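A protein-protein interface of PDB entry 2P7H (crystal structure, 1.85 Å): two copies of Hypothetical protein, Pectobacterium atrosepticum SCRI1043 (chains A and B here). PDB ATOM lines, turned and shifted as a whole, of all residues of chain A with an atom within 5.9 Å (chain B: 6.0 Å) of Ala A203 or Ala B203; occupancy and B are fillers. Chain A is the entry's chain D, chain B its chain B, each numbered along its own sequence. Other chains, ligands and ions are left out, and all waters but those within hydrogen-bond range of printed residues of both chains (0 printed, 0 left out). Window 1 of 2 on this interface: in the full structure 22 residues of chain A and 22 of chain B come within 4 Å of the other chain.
The side-chain hydroxyl (OH) of Tyr A222 is in hydrogen-bond range of the backbone carbonyl oxygen (O) of Ala B203, 2.6 Å away. O of Ala A203 lies within hydrogen-bond range of OH of Tyr B222, 2.8 Å away.
The backbone carbonyl oxygen (O) of Cys B226 is in hydrogen-bond range of the backbone NH (N) of Phe B201 (2.9 Å). O of Leu B204 lies within hydrogen-bond range of NE1 of Trp B209. O of Tyr B222 sits close to SG of Cys B226 (3.6 Å). The backbone carbonyl oxygen of Lys A202 lies close to the backbone NH of Val A147, 3.3 Å away. The indole nitrogen of Trp A209 lies within hydrogen-bond range of the backbone carbonyl oxygen of Leu A204. The backbone NH of Ala A205 is in hydrogen-bond range of the side-chain amide oxygen of Gln A208 (2.8 Å).
Among the printed residues, pairs that only touch across the chains: Val A147 with Phe B201 (3.6 Å), Ile A151 with Tyr B222 (3.7 Å), Ile A151 with Cys B226 (3.98 Å), Phe A201 with Val B147 (3.7 Å), Phe A201 with Phe B201 (3.9 Å), Ala A203 with Ala B203 (3.4 Å), Leu A204 with Tyr B222 (3.7 Å), Gln A208 with Tyr B222 (3.9 Å), Tyr A222 with Ile B151 (3.8 Å), Tyr A222 with Leu B204 (3.6 Å), Tyr A222 with Gln B208 (3.8 Å) and Cys A226 with Ile B151 (3.8 Å).
Ala A203 touches two residues of chain B. Of the printed residues of chain A, Ile B151 touches Tyr A222 (3.8 Å) and Cys A226 (3.8 Å). Ala B203 touches two residues of chain A. Printed residues of chain A within 4 Å of Leu B204: Tyr A222. Ala B205 touches none of the printed residues of chain A. The nearest residue of chain B that does not touch Ala A203 is Phe B201 (4.8 Å). The nearest residue of chain A that does not touch Ala B203 is Phe A201 (4.9 Å). The nearest printed residue of chain B that does not touch Val A147 is Tyr B222 (6.1 Å).
Printed residues of chain B that touch a printed residue of chain A: Val B147, Ile B151, Phe B201, Ala B203, Leu B204, Gln B208, Tyr B222 and Cys B226. Of the 13 printed residues of chain A, 8 touch a printed residue of chain B. Hydrophobic or aromatic side chains of chain A within 4 Å of the printed part of chain B: Val A147, Ile A151, Phe A201, Ala A203, Leu A204 and Tyr A222. Among the printed residues, 14 pairs touch across the chains. Among the printed residues, no Asp or Glu carboxylate lies within 4 Å of a Lys or Arg side-chain nitrogen of the other chain.
Ile A151 touches Tyr B222, and with the chains exchanged Tyr A222 touches Ile B151. Ile A151 touches Cys B226, and with the chains exchanged Cys A226 touches Ile B151. Ala B203 touches its own counterpart, Ala A203. Ala A203 touches Tyr B222, and with the chains exchanged Tyr A222 touches Ala B203. Of the 14 pairs that touch across the chains among the printed residues, 14 have their exchanged pair printed and touching as well.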
ATOM      1  N   VAL A 147      -8.317   6.235   9.843  1.00  0.00           N
ATOM      2  CA  VAL A 147      -8.869   7.207  10.810  1.00  0.00           C
ATOM      3  C   VAL A 147      -8.603   6.774  12.257  1.00  0.00           C
ATOM      4  O   VAL A 147      -8.167   7.579  13.055  1.00  0.00           O
ATOM      5  CB  VAL A 147     -10.355   7.491  10.567  1.00  0.00           C
ATOM      6  CG1 VAL A 147     -10.929   8.392  11.675  1.00  0.00           C
ATOM      7  CG2 VAL A 147     -10.511   8.169   9.223  1.00  0.00           C
ATOM      8  N   SER A 148      -8.892   5.525  12.600  1.00  0.00           N
ATOM      9  CA  SER A 148      -8.712   5.052  13.969  1.00  0.00           C
ATOM     10  C   SER A 148      -7.288   5.251  14.454  1.00  0.00           C
ATOM     11  O   SER A 148      -7.051   5.567  15.618  1.00  0.00           O
ATOM     12  CB  SER A 148      -9.046   3.579  14.057  1.00  0.00           C
ATOM     13  OG  SER A 148      -8.462   2.894  13.008  1.00  0.00           O
ATOM     14  N   ILE A 151      -6.551   8.897  15.081  1.00  0.00           N
ATOM     15  CA  ILE A 151      -7.144   9.309  16.363  1.00  0.00           C
ATOM     16  C   ILE A 151      -6.185   8.852  17.481  1.00  0.00           C
ATOM     17  O   ILE A 151      -5.897   9.636  18.371  1.00  0.00           O
ATOM     18  CB  ILE A 151      -8.601   8.745  16.578  1.00  0.00           C
ATOM     19  CG1 ILE A 151      -9.581   9.420  15.580  1.00  0.00           C
ATOM     20  CG2 ILE A 151      -9.069   8.911  18.040  1.00  0.00           C
ATOM     21  CD1 ILE A 151     -10.870   8.671  15.330  1.00  0.00           C
ATOM     22  N   PHE A 200     -12.251  -0.384   3.513  1.00  0.00           N
ATOM     23  CA  PHE A 200     -13.000  -0.165   4.747  1.00  0.00           C
ATOM     24  C   PHE A 200     -12.681   1.132   5.474  1.00  0.00           C
ATOM     25  O   PHE A 200     -11.636   1.270   6.108  1.00  0.00           O
ATOM     26  CB  PHE A 200     -12.882  -1.345   5.733  1.00  0.00           C
ATOM     27  CG  PHE A 200     -13.961  -1.354   6.779  1.00  0.00           C
ATOM     28  CD1 PHE A 200     -15.205  -1.956   6.525  1.00  0.00           C
ATOM     29  CD2 PHE A 200     -13.770  -0.727   7.963  1.00  0.00           C
ATOM     30  CE1 PHE A 200     -16.187  -1.944   7.468  1.00  0.00           C
ATOM     31  CE2 PHE A 200     -14.754  -0.710   8.919  1.00  0.00           C
ATOM     32  CZ  PHE A 200     -15.973  -1.313   8.661  1.00  0.00           C
ATOM     33  N   PHE A 201     -13.626   2.061   5.452  1.00  0.00           N
ATOM     34  CA  PHE A 201     -13.496   3.315   6.197  1.00  0.00           C
ATOM     35  C   PHE A 201     -13.530   3.024   7.698  1.00  0.00           C
ATOM     36  O   PHE A 201     -14.572   2.651   8.228  1.00  0.00           O
ATOM     37  CB  PHE A 201     -14.594   4.293   5.805  1.00  0.00           C
ATOM     38  CG  PHE A 201     -14.276   5.711   6.143  1.00  0.00           C
ATOM     39  CD1 PHE A 201     -14.380   6.158   7.448  1.00  0.00           C
ATOM     40  CD2 PHE A 201     -13.866   6.603   5.173  1.00  0.00           C
ATOM     41  CE1 PHE A 201     -14.069   7.492   7.767  1.00  0.00           C
ATOM     42  CE2 PHE A 201     -13.607   7.923   5.472  1.00  0.00           C
ATOM     43  CZ  PHE A 201     -13.678   8.355   6.772  1.00  0.00           C
ATOM     44  N   LYS A 202     -12.390   3.170   8.370  1.00  0.00           N
ATOM     45  CA  LYS A 202     -12.250   2.633   9.750  1.00  0.00           C
ATOM     46  C   LYS A 202     -11.970   3.766  10.762  1.00  0.00           C
ATOM     47  O   LYS A 202     -10.858   4.290  10.817  1.00  0.00           O
ATOM     48  CB  LYS A 202     -11.118   1.607   9.805  1.00  0.00           C
ATOM     49  CG  LYS A 202     -10.985   0.842  11.135  1.00  0.00           C
ATOM     50  CD  LYS A 202      -9.535   0.359  11.322  1.00  0.00           C
ATOM     51  CE  LYS A 202      -9.382  -0.564  12.498  1.00  0.00           C
ATOM     52  NZ  LYS A 202      -7.952  -1.032  12.539  1.00  0.00           N
ATOM     53  N   ALA A 203     -12.977   4.119  11.562  1.00  0.00           N
ATOM     54  CA  ALA A 203     -12.821   5.188  12.559  1.00  0.00           C
ATOM     55  C   ALA A 203     -12.710   4.659  13.989  1.00  0.00           C
ATOM     56  O   ALA A 203     -12.424   5.428  14.896  1.00  0.00           O
ATOM     57  CB  ALA A 203     -13.969   6.200  12.410  1.00  0.00           C
ATOM     58  N   LEU A 204     -12.957   3.364  14.192  1.00  0.00           N
ATOM     59  CA  LEU A 204     -12.802   2.701  15.506  1.00  0.00           C
ATOM     60  C   LEU A 204     -11.655   1.702  15.495  1.00  0.00           C
ATOM     61  O   LEU A 204     -11.319   1.148  14.449  1.00  0.00           O
ATOM     62  CB  LEU A 204     -14.081   1.950  15.897  1.00  0.00           C
ATOM     63  CG  LEU A 204     -15.399   2.696  16.119  1.00  0.00           C
ATOM     64  CD1 LEU A 204     -16.547   1.694  16.136  1.00  0.00           C
ATOM     65  CD2 LEU A 204     -15.366   3.456  17.442  1.00  0.00           C
ATOM     66  N   ALA A 205     -11.037   1.482  16.654  1.00  0.00           N
ATOM     67  CA  ALA A 205      -9.963   0.499  16.792  1.00  0.00           C
ATOM     68  C   ALA A 205     -10.544  -0.927  16.789  1.00  0.00           C
ATOM     69  O   ALA A 205     -11.704  -1.125  17.162  1.00  0.00           O
ATOM     70  CB  ALA A 205      -9.163   0.741  18.075  1.00  0.00           C
ATOM     71  N   GLN A 208     -12.235  -1.913  19.788  1.00  0.00           N
ATOM     72  CA  GLN A 208     -13.530  -1.279  19.959  1.00  0.00           C
ATOM     73  C   GLN A 208     -14.538  -1.997  19.072  1.00  0.00           C
ATOM     74  O   GLN A 208     -15.661  -2.275  19.508  1.00  0.00           O
ATOM     75  CB  GLN A 208     -13.455   0.218  19.643  1.00  0.00           C
ATOM     76  CG  GLN A 208     -12.492   0.962  20.574  1.00  0.00           C
ATOM     77  CD  GLN A 208     -12.200   2.377  20.124  1.00  0.00           C
ATOM     78  OE1 GLN A 208     -12.070   2.646  18.924  1.00  0.00           O
ATOM     79  NE2 GLN A 208     -12.075   3.294  21.087  1.00  0.00           N
ATOM     80  N   TRP A 209     -14.124  -2.316  17.843  1.00  0.00           N
ATOM     81  CA  TRP A 209     -14.972  -3.065  16.909  1.00  0.00           C
ATOM     82  C   TRP A 209     -15.401  -4.402  17.511  1.00  0.00           C
ATOM     83  O   TRP A 209     -16.580  -4.749  17.471  1.00  0.00           O
ATOM     84  CB  TRP A 209     -14.240  -3.356  15.604  1.00  0.00           C
ATOM     85  CG  TRP A 209     -14.161  -2.200  14.651  1.00  0.00           C
ATOM     86  CD1 TRP A 209     -13.034  -1.552  14.242  1.00  0.00           C
ATOM     87  CD2 TRP A 209     -15.250  -1.583  13.963  1.00  0.00           C
ATOM     88  NE1 TRP A 209     -13.356  -0.563  13.342  1.00  0.00           N
ATOM     89  CE2 TRP A 209     -14.709  -0.556  13.159  1.00  0.00           C
ATOM     90  CE3 TRP A 209     -16.629  -1.801  13.940  1.00  0.00           C
ATOM     91  CZ2 TRP A 209     -15.506   0.257  12.345  1.00  0.00           C
ATOM     92  CZ3 TRP A 209     -17.412  -1.006  13.124  1.00  0.00           C
ATOM     93  CH2 TRP A 209     -16.853   0.023  12.351  1.00  0.00           C
ATOM     94  N   TYR A 222     -24.411  -1.126   7.820  1.00  0.00           N
ATOM     95  CA  TYR A 222     -23.494  -0.068   8.219  1.00  0.00           C
ATOM     96  C   TYR A 222     -22.102  -0.434   7.747  1.00  0.00           C
ATOM     97  O   TYR A 222     -21.397   0.396   7.180  1.00  0.00           O
ATOM     98  CB  TYR A 222     -23.484   0.183   9.739  1.00  0.00           C
ATOM     99  CG  TYR A 222     -22.433   1.180  10.201  1.00  0.00           C
ATOM    100  CD1 TYR A 222     -22.666   2.537  10.150  1.00  0.00           C
ATOM    101  CD2 TYR A 222     -21.236   0.765  10.722  1.00  0.00           C
ATOM    102  CE1 TYR A 222     -21.714   3.455  10.564  1.00  0.00           C
ATOM    103  CE2 TYR A 222     -20.261   1.683  11.107  1.00  0.00           C
ATOM    104  CZ  TYR A 222     -20.523   3.021  11.049  1.00  0.00           C
ATOM    105  OH  TYR A 222     -19.566   3.928  11.466  1.00  0.00           O
ATOM    106  N   CYS A 226     -19.491   1.439   5.170  1.00  0.00           N
ATOM    107  CA  CYS A 226     -18.104   1.814   5.435  1.00  0.00           C
ATOM    108  C   CYS A 226     -17.190   1.375   4.291  1.00  0.00           C
ATOM    109  O   CYS A 226     -16.178   2.022   4.000  1.00  0.00           O
ATOM    110  CB  CYS A 226     -17.611   1.191   6.757  1.00  0.00           C
ATOM    111  SG  CYS A 226     -18.405   1.892   8.231  1.00  0.00           S
ATOM    112  N   VAL B 147     -19.018  12.106   7.876  1.00  0.00           N
ATOM    113  CA  VAL B 147     -18.813  10.690   7.530  1.00  0.00           C
ATOM    114  C   VAL B 147     -20.057   9.840   7.849  1.00  0.00           C
ATOM    115  O   VAL B 147     -20.506   9.091   6.985  1.00  0.00           O
ATOM    116  CB  VAL B 147     -17.587  10.102   8.194  1.00  0.00           C
ATOM    117  CG1 VAL B 147     -17.568   8.564   8.016  1.00  0.00           C
ATOM    118  CG2 VAL B 147     -16.346  10.756   7.578  1.00  0.00           C
ATOM    119  N   SER B 148     -20.638  10.027   9.022  1.00  0.00           N
ATOM    120  CA  SER B 148     -21.829   9.259   9.424  1.00  0.00           C
ATOM    121  C   SER B 148     -22.993   9.423   8.409  1.00  0.00           C
ATOM    122  O   SER B 148     -23.719   8.434   8.038  1.00  0.00           O
ATOM    123  CB  SER B 148     -22.246   9.685  10.821  1.00  0.00           C
ATOM    124  OG  SER B 148     -22.543  11.059  10.847  1.00  0.00           O
ATOM    125  N   ILE B 151     -22.194   7.668   5.141  1.00  0.00           N
ATOM    126  CA  ILE B 151     -22.396   6.237   5.243  1.00  0.00           C
ATOM    127  C   ILE B 151     -23.907   5.931   5.096  1.00  0.00           C
ATOM    128  O   ILE B 151     -24.312   4.991   4.360  1.00  0.00           O
ATOM    129  CB  ILE B 151     -21.765   5.676   6.569  1.00  0.00           C
ATOM    130  CG1 ILE B 151     -20.238   5.774   6.500  1.00  0.00           C
ATOM    131  CG2 ILE B 151     -22.214   4.199   6.804  1.00  0.00           C
ATOM    132  CD1 ILE B 151     -19.567   5.495   7.885  1.00  0.00           C
ATOM    133  N   PHE B 200     -15.575  18.111  15.177  1.00  0.00           N
ATOM    134  CA  PHE B 200     -15.767  16.681  15.569  1.00  0.00           C
ATOM    135  C   PHE B 200     -15.851  15.679  14.396  1.00  0.00           C
ATOM    136  O   PHE B 200     -16.836  15.623  13.669  1.00  0.00           O
ATOM    137  CB  PHE B 200     -16.961  16.502  16.494  1.00  0.00           C
ATOM    138  CG  PHE B 200     -16.951  15.178  17.219  1.00  0.00           C
ATOM    139  CD1 PHE B 200     -16.228  15.011  18.395  1.00  0.00           C
ATOM    140  CD2 PHE B 200     -17.628  14.089  16.702  1.00  0.00           C
ATOM    141  CE1 PHE B 200     -16.187  13.798  19.022  1.00  0.00           C
ATOM    142  CE2 PHE B 200     -17.597  12.851  17.360  1.00  0.00           C
ATOM    143  CZ  PHE B 200     -16.871  12.717  18.509  1.00  0.00           C
ATOM    144  N   PHE B 201     -14.803  14.878  14.241  1.00  0.00           N
ATOM    145  CA  PHE B 201     -14.771  13.838  13.225  1.00  0.00           C
ATOM    146  C   PHE B 201     -15.809  12.743  13.577  1.00  0.00           C
ATOM    147  O   PHE B 201     -15.617  11.994  14.518  1.00  0.00           O
ATOM    148  CB  PHE B 201     -13.347  13.271  13.089  1.00  0.00           C
ATOM    149  CG  PHE B 201     -13.129  12.502  11.805  1.00  0.00           C
ATOM    150  CD1 PHE B 201     -13.708  11.246  11.628  1.00  0.00           C
ATOM    151  CD2 PHE B 201     -12.397  13.053  10.758  1.00  0.00           C
ATOM    152  CE1 PHE B 201     -13.535  10.549  10.419  1.00  0.00           C
ATOM    153  CE2 PHE B 201     -12.202  12.357   9.545  1.00  0.00           C
ATOM    154  CZ  PHE B 201     -12.760  11.121   9.372  1.00  0.00           C
ATOM    155  N   LYS B 202     -16.906  12.681  12.825  1.00  0.00           N
ATOM    156  CA  LYS B 202     -18.101  11.893  13.212  1.00  0.00           C
ATOM    157  C   LYS B 202     -18.375  10.751  12.236  1.00  0.00           C
ATOM    158  O   LYS B 202     -18.864  10.997  11.129  1.00  0.00           O
ATOM    159  CB  LYS B 202     -19.360  12.811  13.214  1.00  0.00           C
ATOM    160  CG  LYS B 202     -20.643  12.176  13.765  1.00  0.00           C
ATOM    161  CD  LYS B 202     -21.909  12.991  13.373  1.00  0.00           C
ATOM    162  CE  LYS B 202     -23.147  12.496  14.083  1.00  0.00           C
ATOM    163  NZ  LYS B 202     -24.398  13.203  13.568  1.00  0.00           N
ATOM    164  N   ALA B 203     -18.124   9.514  12.659  1.00  0.00           N
ATOM    165  CA  ALA B 203     -18.327   8.355  11.792  1.00  0.00           C
ATOM    166  C   ALA B 203     -19.510   7.490  12.220  1.00  0.00           C
ATOM    167  O   ALA B 203     -19.835   6.518  11.527  1.00  0.00           O
ATOM    168  CB  ALA B 203     -17.058   7.513  11.695  1.00  0.00           C
ATOM    169  N   LEU B 204     -20.125   7.828  13.355  1.00  0.00           N
ATOM    170  CA  LEU B 204     -21.304   7.146  13.855  1.00  0.00           C
ATOM    171  C   LEU B 204     -22.482   8.109  13.926  1.00  0.00           C
ATOM    172  O   LEU B 204     -22.301   9.326  14.085  1.00  0.00           O
ATOM    173  CB  LEU B 204     -21.031   6.613  15.264  1.00  0.00           C
ATOM    174  CG  LEU B 204     -20.047   5.463  15.410  1.00  0.00           C
ATOM    175  CD1 LEU B 204     -19.669   5.247  16.918  1.00  0.00           C
ATOM    176  CD2 LEU B 204     -20.719   4.205  14.835  1.00  0.00           C
ATOM    177  N   ALA B 205     -23.690   7.551  13.808  1.00  0.00           N
ATOM    178  CA  ALA B 205     -24.933   8.318  13.912  1.00  0.00           C
ATOM    179  C   ALA B 205     -25.210   8.655  15.364  1.00  0.00           C
ATOM    180  O   ALA B 205     -24.806   7.905  16.256  1.00  0.00           O
ATOM    181  CB  ALA B 205     -26.097   7.501  13.367  1.00  0.00           C
ATOM    182  N   GLN B 208     -26.424   5.858  17.483  1.00  0.00           N
ATOM    183  CA  GLN B 208     -25.348   4.923  17.799  1.00  0.00           C
ATOM    184  C   GLN B 208     -24.437   5.519  18.878  1.00  0.00           C
ATOM    185  O   GLN B 208     -23.946   4.810  19.753  1.00  0.00           O
ATOM    186  CB  GLN B 208     -24.529   4.577  16.545  1.00  0.00           C
ATOM    187  CG  GLN B 208     -25.352   4.009  15.375  1.00  0.00           C
ATOM    188  CD  GLN B 208     -24.532   3.857  14.080  1.00  0.00           C
ATOM    189  OE1 GLN B 208     -23.736   4.733  13.709  1.00  0.00           O
ATOM    190  NE2 GLN B 208     -24.738   2.747  13.385  1.00  0.00           N
ATOM    191  N   TRP B 209     -24.196   6.823  18.818  1.00  0.00           N
ATOM    192  CA  TRP B 209     -23.408   7.458  19.878  1.00  0.00           C
ATOM    193  C   TRP B 209     -24.145   7.382  21.222  1.00  0.00           C
ATOM    194  O   TRP B 209     -23.556   7.027  22.238  1.00  0.00           O
ATOM    195  CB  TRP B 209     -23.137   8.922  19.564  1.00  0.00           C
ATOM    196  CG  TRP B 209     -22.099   9.182  18.557  1.00  0.00           C
ATOM    197  CD1 TRP B 209     -22.297   9.685  17.313  1.00  0.00           C
ATOM    198  CD2 TRP B 209     -20.680   9.023  18.706  1.00  0.00           C
ATOM    199  NE1 TRP B 209     -21.101   9.846  16.664  1.00  0.00           N
ATOM    200  CE2 TRP B 209     -20.088   9.449  17.499  1.00  0.00           C
ATOM    201  CE3 TRP B 209     -19.854   8.565  19.738  1.00  0.00           C
ATOM    202  CZ2 TRP B 209     -18.711   9.417  17.287  1.00  0.00           C
ATOM    203  CZ3 TRP B 209     -18.489   8.541  19.525  1.00  0.00           C
ATOM    204  CH2 TRP B 209     -17.930   8.963  18.310  1.00  0.00           C
ATOM    205  N   TYR B 222     -10.747   9.485  23.452  1.00  0.00           N
ATOM    206  CA  TYR B 222     -11.139   9.145  22.116  1.00  0.00           C
ATOM    207  C   TYR B 222     -11.920  10.316  21.560  1.00  0.00           C
ATOM    208  O   TYR B 222     -11.650  10.724  20.483  1.00  0.00           O
ATOM    209  CB  TYR B 222     -11.996   7.862  22.043  1.00  0.00           C
ATOM    210  CG  TYR B 222     -12.518   7.551  20.652  1.00  0.00           C
ATOM    211  CD1 TYR B 222     -11.706   6.962  19.694  1.00  0.00           C
ATOM    212  CD2 TYR B 222     -13.815   7.846  20.295  1.00  0.00           C
ATOM    213  CE1 TYR B 222     -12.169   6.686  18.389  1.00  0.00           C
ATOM    214  CE2 TYR B 222     -14.289   7.593  18.990  1.00  0.00           C
ATOM    215  CZ  TYR B 222     -13.456   7.001  18.048  1.00  0.00           C
ATOM    216  OH  TYR B 222     -13.954   6.760  16.761  1.00  0.00           O
ATOM    217  N   CYS B 226     -11.122  12.739  18.296  1.00  0.00           N
ATOM    218  CA  CYS B 226     -12.021  12.992  17.190  1.00  0.00           C
ATOM    219  C   CYS B 226     -12.162  14.487  16.909  1.00  0.00           C
ATOM    220  O   CYS B 226     -12.354  14.909  15.778  1.00  0.00           O
ATOM    221  CB  CYS B 226     -13.424  12.443  17.494  1.00  0.00           C
ATOM    222  SG  CYS B 226     -13.577  10.638  17.492  1.00  0.00           S
